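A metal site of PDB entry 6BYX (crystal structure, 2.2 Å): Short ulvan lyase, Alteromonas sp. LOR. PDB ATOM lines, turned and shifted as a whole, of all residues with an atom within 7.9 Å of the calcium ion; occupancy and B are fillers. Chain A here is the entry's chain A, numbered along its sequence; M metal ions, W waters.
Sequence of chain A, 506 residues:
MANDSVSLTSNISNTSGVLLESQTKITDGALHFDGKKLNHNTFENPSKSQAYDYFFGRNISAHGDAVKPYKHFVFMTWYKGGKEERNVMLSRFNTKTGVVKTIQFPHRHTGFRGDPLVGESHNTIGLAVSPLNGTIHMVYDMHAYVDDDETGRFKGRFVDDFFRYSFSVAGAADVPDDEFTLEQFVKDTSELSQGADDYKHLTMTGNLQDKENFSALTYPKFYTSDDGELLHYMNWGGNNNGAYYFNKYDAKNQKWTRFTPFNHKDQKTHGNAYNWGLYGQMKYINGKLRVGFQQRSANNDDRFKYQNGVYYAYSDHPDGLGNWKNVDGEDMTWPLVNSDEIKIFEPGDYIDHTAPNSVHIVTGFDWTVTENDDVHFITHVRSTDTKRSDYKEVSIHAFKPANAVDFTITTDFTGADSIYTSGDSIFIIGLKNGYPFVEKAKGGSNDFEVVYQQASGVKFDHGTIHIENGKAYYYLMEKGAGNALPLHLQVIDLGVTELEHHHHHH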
ATOM      1  N   VAL A 159     -12.230  19.607  -7.336  1.00  0.00           N
ATOM      2  CA  VAL A 159     -11.506  20.858  -7.544  1.00  0.00           C
ATOM      3  C   VAL A 159     -10.209  20.808  -6.755  1.00  0.00           C
ATOM      4  O   VAL A 159     -10.205  20.479  -5.573  1.00  0.00           O
ATOM      5  CB  VAL A 159     -12.375  22.043  -7.130  1.00  0.00           C
ATOM      6  CG1 VAL A 159     -11.554  23.313  -7.175  1.00  0.00           C
ATOM      7  CG2 VAL A 159     -13.599  22.146  -8.035  1.00  0.00           C
ATOM      8  N   ASP A 160      -9.096  21.117  -7.423  1.00  0.00           N
ATOM      9  CA  ASP A 160      -7.784  21.102  -6.806  1.00  0.00           C
ATOM     10  C   ASP A 160      -7.378  19.723  -6.328  1.00  0.00           C
ATOM     11  O   ASP A 160      -6.448  19.607  -5.526  1.00  0.00           O
ATOM     12  CB  ASP A 160      -7.699  22.057  -5.622  1.00  0.00           C
ATOM     13  CG  ASP A 160      -8.202  23.419  -5.946  1.00  0.00           C
ATOM     14  OD1 ASP A 160      -7.879  23.925  -7.032  1.00  0.00           O
ATOM     15  OD2 ASP A 160      -8.906  23.988  -5.078  1.00  0.00           O
ATOM     16  N   ASP A 161      -8.066  18.662  -6.781  1.00  0.00           N
ATOM     17  CA  ASP A 161      -7.822  17.339  -6.244  1.00  0.00           C
ATOM     18  C   ASP A 161      -8.240  16.271  -7.251  1.00  0.00           C
ATOM     19  O   ASP A 161      -8.721  15.201  -6.858  1.00  0.00           O
ATOM     20  CB  ASP A 161      -8.564  17.151  -4.920  1.00  0.00           C
ATOM     21  CG  ASP A 161      -8.115  15.894  -4.152  1.00  0.00           C
ATOM     22  OD1 ASP A 161      -6.886  15.727  -3.935  1.00  0.00           O
ATOM     23  OD2 ASP A 161      -8.991  15.084  -3.739  1.00  0.00           O
ATOM     24  N   PHE A 162      -8.041  16.544  -8.531  1.00  0.00           N
ATOM     25  CA  PHE A 162      -8.429  15.618  -9.578  1.00  0.00           C
ATOM     26  C   PHE A 162      -7.319  14.641  -9.972  1.00  0.00           C
ATOM     27  O   PHE A 162      -7.595  13.691 -10.706  1.00  0.00           O
ATOM     28  CB  PHE A 162      -8.906  16.404 -10.797  1.00  0.00           C
ATOM     29  CG  PHE A 162      -7.954  17.468 -11.246  1.00  0.00           C
ATOM     30  CD1 PHE A 162      -6.780  17.131 -11.908  1.00  0.00           C
ATOM     31  CD2 PHE A 162      -8.206  18.807 -10.999  1.00  0.00           C
ATOM     32  CE1 PHE A 162      -5.895  18.106 -12.327  1.00  0.00           C
ATOM     33  CE2 PHE A 162      -7.323  19.776 -11.402  1.00  0.00           C
ATOM     34  CZ  PHE A 162      -6.160  19.424 -12.077  1.00  0.00           C
ATOM     35  N   PHE A 163      -6.098  14.851  -9.480  1.00  0.00           N
ATOM     36  CA  PHE A 163      -4.998  13.915  -9.634  1.00  0.00           C
ATOM     37  C   PHE A 163      -4.381  13.748  -8.246  1.00  0.00           C
ATOM     38  O   PHE A 163      -3.953  14.735  -7.649  1.00  0.00           O
ATOM     39  CB  PHE A 163      -3.965  14.455 -10.641  1.00  0.00           C
ATOM     40  CG  PHE A 163      -2.814  13.519 -10.908  1.00  0.00           C
ATOM     41  CD1 PHE A 163      -1.741  13.441 -10.045  1.00  0.00           C
ATOM     42  CD2 PHE A 163      -2.796  12.732 -12.059  1.00  0.00           C
ATOM     43  CE1 PHE A 163      -0.658  12.595 -10.273  1.00  0.00           C
ATOM     44  CE2 PHE A 163      -1.719  11.853 -12.311  1.00  0.00           C
ATOM     45  CZ  PHE A 163      -0.646  11.798 -11.391  1.00  0.00           C
ATOM     46  N   ARG A 164      -4.331  12.510  -7.742  1.00  0.00           N
ATOM     47  CA  ARG A 164      -4.023  12.260  -6.321  1.00  0.00           C
ATOM     48  C   ARG A 164      -2.721  11.474  -6.192  1.00  0.00           C
ATOM     49  O   ARG A 164      -2.691  10.251  -6.356  1.00  0.00           O
ATOM     50  CB  ARG A 164      -5.189  11.546  -5.660  1.00  0.00           C
ATOM     51  CG  ARG A 164      -6.457  12.358  -5.761  1.00  0.00           C
ATOM     52  CD  ARG A 164      -7.699  11.615  -5.342  1.00  0.00           C
ATOM     53  NE  ARG A 164      -8.774  12.559  -5.074  1.00  0.00           N
ATOM     54  CZ  ARG A 164     -10.045  12.229  -4.867  1.00  0.00           C
ATOM     55  NH1 ARG A 164     -10.427  10.945  -4.883  1.00  0.00           N
ATOM     56  NH2 ARG A 164     -10.930  13.192  -4.591  1.00  0.00           N
ATOM     57  N   TYR A 165      -1.647  12.195  -5.874  1.00  0.00           N
ATOM     58  CA  TYR A 165      -0.292  11.659  -5.789  1.00  0.00           C
ATOM     59  C   TYR A 165       0.244  11.849  -4.375  1.00  0.00           C
ATOM     60  O   TYR A 165       0.235  12.960  -3.841  1.00  0.00           O
ATOM     61  CB  TYR A 165       0.597  12.359  -6.822  1.00  0.00           C
ATOM     62  CG  TYR A 165       2.084  12.038  -6.787  1.00  0.00           C
ATOM     63  CD1 TYR A 165       2.531  10.748  -6.631  1.00  0.00           C
ATOM     64  CD2 TYR A 165       3.041  13.045  -6.976  1.00  0.00           C
ATOM     65  CE1 TYR A 165       3.901  10.449  -6.614  1.00  0.00           C
ATOM     66  CE2 TYR A 165       4.410  12.763  -6.972  1.00  0.00           C
ATOM     67  CZ  TYR A 165       4.836  11.466  -6.785  1.00  0.00           C
ATOM     68  OH  TYR A 165       6.175  11.187  -6.768  1.00  0.00           O
ATOM     69  N   LYS A 187       3.677  16.459   2.625  1.00  0.00           N
ATOM     70  CA  LYS A 187       2.365  17.102   2.621  1.00  0.00           C
ATOM     71  C   LYS A 187       2.225  18.009   1.401  1.00  0.00           C
ATOM     72  O   LYS A 187       3.201  18.470   0.809  1.00  0.00           O
ATOM     73  CB  LYS A 187       2.159  17.916   3.914  1.00  0.00           C
ATOM     74  CG  LYS A 187       1.989  17.058   5.184  1.00  0.00           C
ATOM     75  CD  LYS A 187       1.579  17.913   6.367  1.00  0.00           C
ATOM     76  CE  LYS A 187       1.148  17.094   7.558  1.00  0.00           C
ATOM     77  NZ  LYS A 187       0.951  17.978   8.765  1.00  0.00           N
ATOM     78  N   ASP A 188       0.969  18.282   1.040  1.00  0.00           N
ATOM     79  CA  ASP A 188       0.678  19.330   0.063  1.00  0.00           C
ATOM     80  C   ASP A 188       0.651  20.658   0.825  1.00  0.00           C
ATOM     81  O   ASP A 188      -0.279  20.938   1.594  1.00  0.00           O
ATOM     82  CB  ASP A 188      -0.635  19.017  -0.643  1.00  0.00           C
ATOM     83  CG  ASP A 188      -1.061  20.109  -1.628  1.00  0.00           C
ATOM     84  OD1 ASP A 188      -0.404  21.168  -1.733  1.00  0.00           O
ATOM     85  OD2 ASP A 188      -2.069  19.885  -2.334  1.00  0.00           O
ATOM     86  N   THR A 189       1.699  21.446   0.646  1.00  0.00           N
ATOM     87  CA  THR A 189       1.770  22.792   1.192  1.00  0.00           C
ATOM     88  C   THR A 189       1.775  23.855   0.110  1.00  0.00           C
ATOM     89  O   THR A 189       2.290  24.955   0.316  1.00  0.00           O
ATOM     90  CB  THR A 189       3.000  22.945   2.090  1.00  0.00           C
ATOM     91  OG1 THR A 189       4.185  22.751   1.303  1.00  0.00           O
ATOM     92  CG2 THR A 189       2.974  21.978   3.255  1.00  0.00           C
ATOM     93  N   SER A 190       1.193  23.554  -1.052  1.00  0.00           N
ATOM     94  CA  SER A 190       1.046  24.521  -2.130  1.00  0.00           C
ATOM     95  C   SER A 190      -0.123  25.450  -1.857  1.00  0.00           C
ATOM     96  O   SER A 190      -0.877  25.282  -0.887  1.00  0.00           O
ATOM     97  CB  SER A 190       0.819  23.811  -3.462  1.00  0.00           C
ATOM     98  OG  SER A 190      -0.524  23.337  -3.553  1.00  0.00           O
ATOM     99  N   LEU A 192      -2.789  25.508  -3.302  1.00  0.00           N
ATOM    100  CA  LEU A 192      -4.033  24.767  -3.422  1.00  0.00           C
ATOM    101  C   LEU A 192      -4.254  23.782  -2.279  1.00  0.00           C
ATOM    102  O   LEU A 192      -5.354  23.231  -2.163  1.00  0.00           O
ATOM    103  CB  LEU A 192      -4.096  24.029  -4.772  1.00  0.00           C
ATOM    104  CG  LEU A 192      -4.097  24.880  -6.049  1.00  0.00           C
ATOM    105  CD1 LEU A 192      -4.260  24.038  -7.293  1.00  0.00           C
ATOM    106  CD2 LEU A 192      -5.160  25.969  -6.029  1.00  0.00           C
ATOM    107  N   SER A 193      -3.254  23.568  -1.426  1.00  0.00           N
ATOM    108  CA  SER A 193      -3.368  22.638  -0.304  1.00  0.00           C
ATOM    109  C   SER A 193      -4.721  22.803   0.394  1.00  0.00           C
ATOM    110  O   SER A 193      -5.229  23.920   0.534  1.00  0.00           O
ATOM    111  CB  SER A 193      -2.237  22.871   0.691  1.00  0.00           C
ATOM    112  OG  SER A 193      -2.388  22.058   1.844  1.00  0.00           O
ATOM    113  N   GLN A 194      -5.277  21.681   0.865  1.00  0.00           N
ATOM    114  CA  GLN A 194      -6.581  21.707   1.510  1.00  0.00           C
ATOM    115  C   GLN A 194      -6.484  21.557   3.023  1.00  0.00           C
ATOM    116  O   GLN A 194      -7.516  21.375   3.682  1.00  0.00           O
ATOM    117  CB  GLN A 194      -7.478  20.574   0.964  1.00  0.00           C
ATOM    118  CG  GLN A 194      -7.714  20.625  -0.543  1.00  0.00           C
ATOM    119  CD  GLN A 194      -8.576  19.482  -1.035  1.00  0.00           C
ATOM    120  OE1 GLN A 194      -8.406  18.343  -0.621  1.00  0.00           O
ATOM    121  NE2 GLN A 194      -9.498  19.788  -1.946  1.00  0.00           N
ATOM    122  N   GLY A 195      -5.303  21.717   3.603  1.00  0.00           N
ATOM    123  CA  GLY A 195      -5.174  21.655   5.052  1.00  0.00           C
ATOM    124  C   GLY A 195      -3.995  20.803   5.493  1.00  0.00           C
ATOM    125  O   GLY A 195      -3.228  20.276   4.690  1.00  0.00           O
ATOM    126  N   ASP A 197      -3.846  17.871   6.878  1.00  0.00           N
ATOM    127  CA  ASP A 197      -3.895  16.438   6.574  1.00  0.00           C
ATOM    128  C   ASP A 197      -3.843  16.174   5.069  1.00  0.00           C
ATOM    129  O   ASP A 197      -4.145  15.047   4.631  1.00  0.00           O
ATOM    130  CB  ASP A 197      -5.134  15.774   7.218  1.00  0.00           C
ATOM    131  CG  ASP A 197      -6.463  16.339   6.733  1.00  0.00           C
ATOM    132  OD1 ASP A 197      -6.483  17.426   6.111  1.00  0.00           O
ATOM    133  OD2 ASP A 197      -7.497  15.707   7.034  1.00  0.00           O
ATOM    134  N   ASP A 198      -3.502  17.186   4.288  1.00  0.00           N
ATOM    135  CA  ASP A 198      -3.440  17.081   2.829  1.00  0.00           C
ATOM    136  C   ASP A 198      -2.103  16.460   2.425  1.00  0.00           C
ATOM    137  O   ASP A 198      -1.060  17.121   2.495  1.00  0.00           O
ATOM    138  CB  ASP A 198      -3.613  18.469   2.218  1.00  0.00           C
ATOM    139  CG  ASP A 198      -3.729  18.420   0.710  1.00  0.00           C
ATOM    140  OD1 ASP A 198      -3.476  17.343   0.133  1.00  0.00           O
ATOM    141  OD2 ASP A 198      -4.078  19.479   0.121  1.00  0.00           O
ATOM    142  N   TYR A 199      -2.134  15.192   1.980  1.00  0.00           N
ATOM    143  CA  TYR A 199      -0.972  14.472   1.451  1.00  0.00           C
ATOM    144  C   TYR A 199      -1.077  14.204  -0.051  1.00  0.00           C
ATOM    145  O   TYR A 199      -0.266  13.439  -0.595  1.00  0.00           O
ATOM    146  CB  TYR A 199      -0.787  13.127   2.179  1.00  0.00           C
ATOM    147  CG  TYR A 199      -0.073  13.227   3.507  1.00  0.00           C
ATOM    148  CD1 TYR A 199      -0.772  13.449   4.690  1.00  0.00           C
ATOM    149  CD2 TYR A 199       1.315  13.090   3.569  1.00  0.00           C
ATOM    150  CE1 TYR A 199      -0.107  13.540   5.906  1.00  0.00           C
ATOM    151  CE2 TYR A 199       1.993  13.196   4.774  1.00  0.00           C
ATOM    152  CZ  TYR A 199       1.280  13.409   5.938  1.00  0.00           C
ATOM    153  OH  TYR A 199       1.966  13.519   7.140  1.00  0.00           O
ATOM    154  N   LYS A 200      -2.055  14.811  -0.716  1.00  0.00           N
ATOM    155  CA  LYS A 200      -2.358  14.561  -2.118  1.00  0.00           C
ATOM    156  C   LYS A 200      -1.822  15.718  -2.954  1.00  0.00           C
ATOM    157  O   LYS A 200      -2.251  16.867  -2.781  1.00  0.00           O
ATOM    158  CB  LYS A 200      -3.870  14.417  -2.304  1.00  0.00           C
ATOM    159  CG  LYS A 200      -4.448  13.178  -1.615  1.00  0.00           C
ATOM    160  CD  LYS A 200      -5.939  13.119  -1.837  1.00  0.00           C
ATOM    161  CE  LYS A 200      -6.616  14.251  -1.046  1.00  0.00           C
ATOM    162  NZ  LYS A 200      -8.099  14.175  -1.074  1.00  0.00           N
ATOM    163  N   HIS A 201      -0.822  15.425  -3.792  1.00  0.00           N
ATOM    164  CA  HIS A 201      -0.286  16.415  -4.719  1.00  0.00           C
ATOM    165  C   HIS A 201      -1.013  16.343  -6.054  1.00  0.00           C
ATOM    166  O   HIS A 201      -1.341  15.260  -6.544  1.00  0.00           O
ATOM    167  CB  HIS A 201       1.218  16.213  -4.915  1.00  0.00           C
ATOM    168  CG  HIS A 201       1.965  16.256  -3.623  1.00  0.00           C
ATOM    169  ND1 HIS A 201       2.587  17.401  -3.162  1.00  0.00           N
ATOM    170  CD2 HIS A 201       2.104  15.322  -2.653  1.00  0.00           C
ATOM    171  CE1 HIS A 201       3.117  17.158  -1.971  1.00  0.00           C
ATOM    172  NE2 HIS A 201       2.841  15.900  -1.635  1.00  0.00           N
ATOM    173  N   LEU A 202      -1.222  17.531  -6.646  1.00  0.00           N
ATOM    174  CA  LEU A 202      -1.984  17.670  -7.869  1.00  0.00           C
ATOM    175  C   LEU A 202      -1.154  17.371  -9.092  1.00  0.00           C
ATOM    176  O   LEU A 202      -1.730  17.109 -10.160  1.00  0.00           O
ATOM    177  CB  LEU A 202      -2.536  19.092  -8.011  1.00  0.00           C
ATOM    178  CG  LEU A 202      -4.021  19.356  -8.324  1.00  0.00           C
ATOM    179  CD1 LEU A 202      -4.217  20.663  -9.121  1.00  0.00           C
ATOM    180  CD2 LEU A 202      -4.739  18.229  -8.997  1.00  0.00           C
ATOM    181  N   LEU A 208       2.507  23.435 -10.110  1.00  0.00           N
ATOM    182  CA  LEU A 208       1.070  23.511 -10.344  1.00  0.00           C
ATOM    183  C   LEU A 208       0.720  24.018 -11.745  1.00  0.00           C
ATOM    184  O   LEU A 208      -0.416  23.808 -12.195  1.00  0.00           O
ATOM    185  CB  LEU A 208       0.415  24.393  -9.272  1.00  0.00           C
ATOM    186  CG  LEU A 208       0.343  23.741  -7.908  1.00  0.00           C
ATOM    187  CD1 LEU A 208      -0.191  24.710  -6.844  1.00  0.00           C
ATOM    188  CD2 LEU A 208      -0.532  22.512  -7.997  1.00  0.00           C
HETATM  189 CA    CA M   1      -3.942  18.465  -2.188  1.00  0.00          CA
HETATM  190  O   HOH W   1      -6.071  17.424  -2.226  1.00  0.00           O
HETATM  191  O   HOH W   2      -4.150  18.336  -4.732  1.00  0.00           O
HETATM  192  O   HOH W   3      -5.619  20.645  -2.759  1.00  0.00           O
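The nearest printed residue that does not touch the calcium ion is Asp 160 (4.3 Å).
Water W1 lies within hydrogen-bond range of the side-chain carboxylate (OD1) of Asp 161 (2.5 Å) and the side-chain amide oxygen (OE1) of Gln 194 (3.0 Å).
Water W3 bridges O of Leu 192 and O of Asp 160.
The calcium ion is bound by OD2 of Asp 188 (2.4 Å), water W1 (2.4 Å), O of Lys 200 (2.4 Å), OD2 of Asp 198 (2.5 Å), water W2 (2.6 Å), OD1 of Asp 198 (2.6 Å) and water W3 (2.8 Å).
The calcium ion has seven donor atoms within binding distance.
The backbone NH (N) of Gln 194 lies close to the side-chain carboxylate (OD2) of Asp 198 (2.6 Å).
NZ of Lys 200 is in salt-bridge range of OD2 of Asp 161 (3.0 Å).
The backbone carbonyl oxygen (O) of Asp 188 lies within hydrogen-bond range of the side-chain hydroxyl (OG) of Ser 193 (2.4 Å).
OD1 of Asp 188 is in hydrogen-bond range of OG of Ser 190 (2.8 Å).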
